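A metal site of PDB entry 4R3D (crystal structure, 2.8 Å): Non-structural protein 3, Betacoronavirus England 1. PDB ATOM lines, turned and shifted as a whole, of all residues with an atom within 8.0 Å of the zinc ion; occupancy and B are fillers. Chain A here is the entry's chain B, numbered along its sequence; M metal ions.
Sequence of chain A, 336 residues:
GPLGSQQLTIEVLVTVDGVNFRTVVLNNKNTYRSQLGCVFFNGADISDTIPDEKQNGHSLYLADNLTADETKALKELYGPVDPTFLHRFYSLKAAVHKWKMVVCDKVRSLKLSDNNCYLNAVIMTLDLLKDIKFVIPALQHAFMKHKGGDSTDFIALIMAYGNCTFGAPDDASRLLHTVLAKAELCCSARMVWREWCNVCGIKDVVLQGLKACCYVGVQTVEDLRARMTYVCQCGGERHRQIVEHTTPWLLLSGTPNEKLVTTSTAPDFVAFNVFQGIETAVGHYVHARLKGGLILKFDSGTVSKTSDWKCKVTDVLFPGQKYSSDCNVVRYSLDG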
ATOM      1  N   TRP A 196       0.704  13.042  22.282  1.00  0.00           N
ATOM      2  CA  TRP A 196       1.013  14.335  21.695  1.00  0.00           C
ATOM      3  C   TRP A 196      -0.017  15.403  22.000  1.00  0.00           C
ATOM      4  O   TRP A 196      -1.202  15.105  22.105  1.00  0.00           O
ATOM      5  CB  TRP A 196       1.291  14.246  20.180  1.00  0.00           C
ATOM      6  CG  TRP A 196       0.117  13.824  19.310  1.00  0.00           C
ATOM      7  CD1 TRP A 196      -0.704  14.628  18.574  1.00  0.00           C
ATOM      8  CD2 TRP A 196      -0.337  12.476  19.077  1.00  0.00           C
ATOM      9  NE1 TRP A 196      -1.638  13.878  17.899  1.00  0.00           N
ATOM     10  CE2 TRP A 196      -1.439  12.543  18.197  1.00  0.00           C
ATOM     11  CE3 TRP A 196       0.079  11.213  19.530  1.00  0.00           C
ATOM     12  CZ2 TRP A 196      -2.130  11.415  17.764  1.00  0.00           C
ATOM     13  CZ3 TRP A 196      -0.612  10.084  19.098  1.00  0.00           C
ATOM     14  CH2 TRP A 196      -1.700  10.189  18.222  1.00  0.00           C
ATOM     15  N   CYS A 197       0.458  16.629  22.204  1.00  0.00           N
ATOM     16  CA  CYS A 197      -0.377  17.816  22.364  1.00  0.00           C
ATOM     17  C   CYS A 197       0.243  18.931  21.523  1.00  0.00           C
ATOM     18  O   CYS A 197       1.465  18.947  21.338  1.00  0.00           O
ATOM     19  CB  CYS A 197      -0.453  18.234  23.827  1.00  0.00           C
ATOM     20  SG  CYS A 197      -1.094  19.893  24.103  1.00  0.00           S
ATOM     21  N   ASN A 198      -0.573  19.846  20.996  1.00  0.00           N
ATOM     22  CA  ASN A 198      -0.023  20.912  20.157  1.00  0.00           C
ATOM     23  C   ASN A 198       0.807  21.958  20.913  1.00  0.00           C
ATOM     24  O   ASN A 198       1.576  22.697  20.315  1.00  0.00           O
ATOM     25  CB  ASN A 198      -1.121  21.601  19.350  1.00  0.00           C
ATOM     26  CG  ASN A 198      -1.596  20.736  18.178  1.00  0.00           C
ATOM     27  OD1 ASN A 198      -1.014  19.680  17.892  1.00  0.00           O
ATOM     28  ND2 ASN A 198      -2.640  21.196  17.496  1.00  0.00           N
ATOM     29  N   VAL A 199       0.663  21.979  22.240  1.00  0.00           N
ATOM     30  CA  VAL A 199       1.377  22.901  23.124  1.00  0.00           C
ATOM     31  C   VAL A 199       2.573  22.242  23.832  1.00  0.00           C
ATOM     32  O   VAL A 199       3.694  22.779  23.797  1.00  0.00           O
ATOM     33  CB  VAL A 199       0.403  23.439  24.211  1.00  0.00           C
ATOM     34  CG1 VAL A 199       1.152  24.273  25.261  1.00  0.00           C
ATOM     35  CG2 VAL A 199      -0.725  24.215  23.564  1.00  0.00           C
ATOM     36  N   CYS A 200       2.312  21.079  24.436  1.00  0.00           N
ATOM     37  CA  CYS A 200       3.289  20.366  25.274  1.00  0.00           C
ATOM     38  C   CYS A 200       4.308  19.582  24.463  1.00  0.00           C
ATOM     39  O   CYS A 200       5.379  19.241  24.976  1.00  0.00           O
ATOM     40  CB  CYS A 200       2.598  19.400  26.242  1.00  0.00           C
ATOM     41  SG  CYS A 200       1.495  20.101  27.515  1.00  0.00           S
ATOM     42  N   GLY A 201       3.960  19.259  23.216  1.00  0.00           N
ATOM     43  CA  GLY A 201       4.833  18.471  22.358  1.00  0.00           C
ATOM     44  C   GLY A 201       4.565  16.967  22.387  1.00  0.00           C
ATOM     45  O   GLY A 201       3.477  16.509  22.789  1.00  0.00           O
ATOM     46  N   VAL A 231      -7.878  15.099  28.144  1.00  0.00           N
ATOM     47  CA  VAL A 231      -7.447  16.472  28.420  1.00  0.00           C
ATOM     48  C   VAL A 231      -6.033  16.523  28.989  1.00  0.00           C
ATOM     49  O   VAL A 231      -5.737  15.844  30.001  1.00  0.00           O
ATOM     50  CB  VAL A 231      -8.445  17.209  29.365  1.00  0.00           C
ATOM     51  CG1 VAL A 231      -7.940  18.622  29.696  1.00  0.00           C
ATOM     52  CG2 VAL A 231      -9.845  17.257  28.731  1.00  0.00           C
ATOM     53  N   CYS A 232      -5.173  17.320  28.353  1.00  0.00           N
ATOM     54  CA  CYS A 232      -3.773  17.449  28.779  1.00  0.00           C
ATOM     55  C   CYS A 232      -3.660  18.261  30.058  1.00  0.00           C
ATOM     56  O   CYS A 232      -4.525  19.075  30.365  1.00  0.00           O
ATOM     57  CB  CYS A 232      -2.909  18.128  27.718  1.00  0.00           C
ATOM     58  SG  CYS A 232      -1.136  18.283  28.209  1.00  0.00           S
ATOM     59  N   GLN A 233      -2.566  18.056  30.786  1.00  0.00           N
ATOM     60  CA  GLN A 233      -2.306  18.820  32.016  1.00  0.00           C
ATOM     61  C   GLN A 233      -2.166  20.335  31.771  1.00  0.00           C
ATOM     62  O   GLN A 233      -2.066  21.108  32.726  1.00  0.00           O
ATOM     63  CB  GLN A 233      -1.050  18.250  32.704  1.00  0.00           C
ATOM     64  CG  GLN A 233      -1.221  16.787  33.131  1.00  0.00           C
ATOM     65  CD  GLN A 233      -2.386  16.575  34.095  1.00  0.00           C
ATOM     66  OE1 GLN A 233      -2.281  16.876  35.283  1.00  0.00           O
ATOM     67  NE2 GLN A 233      -3.513  16.079  33.571  1.00  0.00           N
ATOM     68  N   CYS A 234      -2.170  20.768  30.509  1.00  0.00           N
ATOM     69  CA  CYS A 234      -2.132  22.183  30.165  1.00  0.00           C
ATOM     70  C   CYS A 234      -3.552  22.671  29.835  1.00  0.00           C
ATOM     71  O   CYS A 234      -3.772  23.845  29.513  1.00  0.00           O
ATOM     72  CB  CYS A 234      -1.196  22.443  28.980  1.00  0.00           C
ATOM     73  SG  CYS A 234      -1.885  22.116  27.328  1.00  0.00           S
ATOM     74  N   GLY A 235      -4.508  21.753  29.855  1.00  0.00           N
ATOM     75  CA  GLY A 235      -5.910  22.077  29.663  1.00  0.00           C
ATOM     76  C   GLY A 235      -6.350  21.998  28.206  1.00  0.00           C
ATOM     77  O   GLY A 235      -7.523  22.180  27.885  1.00  0.00           O
ATOM     78  N   GLY A 236      -5.410  21.724  27.324  1.00  0.00           N
ATOM     79  CA  GLY A 236      -5.722  21.571  25.909  1.00  0.00           C
ATOM     80  C   GLY A 236      -6.073  20.126  25.552  1.00  0.00           C
ATOM     81  O   GLY A 236      -6.348  19.278  26.412  1.00  0.00           O
ATOM     82  N   GLU A 237      -6.046  19.843  24.259  1.00  0.00           N
ATOM     83  CA  GLU A 237      -6.366  18.524  23.756  1.00  0.00           C
ATOM     84  C   GLU A 237      -5.088  17.665  23.615  1.00  0.00           C
ATOM     85  O   GLU A 237      -4.086  18.113  23.040  1.00  0.00           O
ATOM     86  CB  GLU A 237      -7.118  18.661  22.419  1.00  0.00           C
ATOM     87  CG  GLU A 237      -7.970  17.486  22.056  1.00  0.00           C
ATOM     88  CD  GLU A 237      -8.758  17.725  20.786  1.00  0.00           C
ATOM     89  OE1 GLU A 237      -8.169  18.206  19.792  1.00  0.00           O
ATOM     90  OE2 GLU A 237      -9.980  17.462  20.805  1.00  0.00           O
ATOM     91  N   ARG A 238      -5.116  16.463  24.198  1.00  0.00           N
ATOM     92  CA  ARG A 238      -3.976  15.549  24.214  1.00  0.00           C
ATOM     93  C   ARG A 238      -4.395  14.218  23.588  1.00  0.00           C
ATOM     94  O   ARG A 238      -5.548  13.807  23.724  1.00  0.00           O
ATOM     95  CB  ARG A 238      -3.459  15.345  25.654  1.00  0.00           C
ATOM     96  CG  ARG A 238      -2.460  14.183  25.836  1.00  0.00           C
ATOM     97  CD  ARG A 238      -1.604  14.329  27.089  1.00  0.00           C
ATOM     98  NE  ARG A 238      -0.354  15.016  26.776  1.00  0.00           N
ATOM     99  CZ  ARG A 238       0.852  14.450  26.819  1.00  0.00           C
ATOM    100  NH1 ARG A 238       0.962  13.192  27.194  1.00  0.00           N
ATOM    101  NH2 ARG A 238       1.938  15.156  26.494  1.00  0.00           N
ATOM    102  N   HIS A 239      -3.486  13.569  22.874  1.00  0.00           N
ATOM    103  CA  HIS A 239      -3.782  12.290  22.237  1.00  0.00           C
ATOM    104  C   HIS A 239      -2.787  11.197  22.635  1.00  0.00           C
ATOM    105  O   HIS A 239      -1.668  11.485  23.042  1.00  0.00           O
ATOM    106  CB  HIS A 239      -3.794  12.437  20.718  1.00  0.00           C
ATOM    107  CG  HIS A 239      -4.723  13.508  20.218  1.00  0.00           C
ATOM    108  ND1 HIS A 239      -5.993  13.228  19.761  1.00  0.00           N
ATOM    109  CD2 HIS A 239      -4.566  14.849  20.100  1.00  0.00           C
ATOM    110  CE1 HIS A 239      -6.568  14.348  19.361  1.00  0.00           C
ATOM    111  NE2 HIS A 239      -5.729  15.344  19.571  1.00  0.00           N
HETATM  112 ZN    ZN M   1      -0.751  20.018  26.398  1.00  0.00          ZN
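The side-chain sulfur (SG) of Cys 197 sits close to the backbone NH (N) of Val 199.
The side-chain sulfur (SG) of Cys 197 sits close to the backbone carbonyl oxygen (O) of Glu 237 (3.6 Å).
The side-chain sulfur of Cys 232 sits close to the guanidinium group of Arg 238, 3.7 Å away.
The side-chain sulfur of Cys 234 lies close to the backbone NH of Gly 236 (3.5 Å).
Of the 15 residues printed, 4 come within 4 Å of the zinc ion.
The zinc ion is bound by SG of Cys 197 (2.3 Å), SG of Cys 200 (2.5 Å), SG of Cys 232 (2.5 Å) and SG of Cys 234 (2.6 Å).
The zinc ion has four donor atoms within binding distance.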
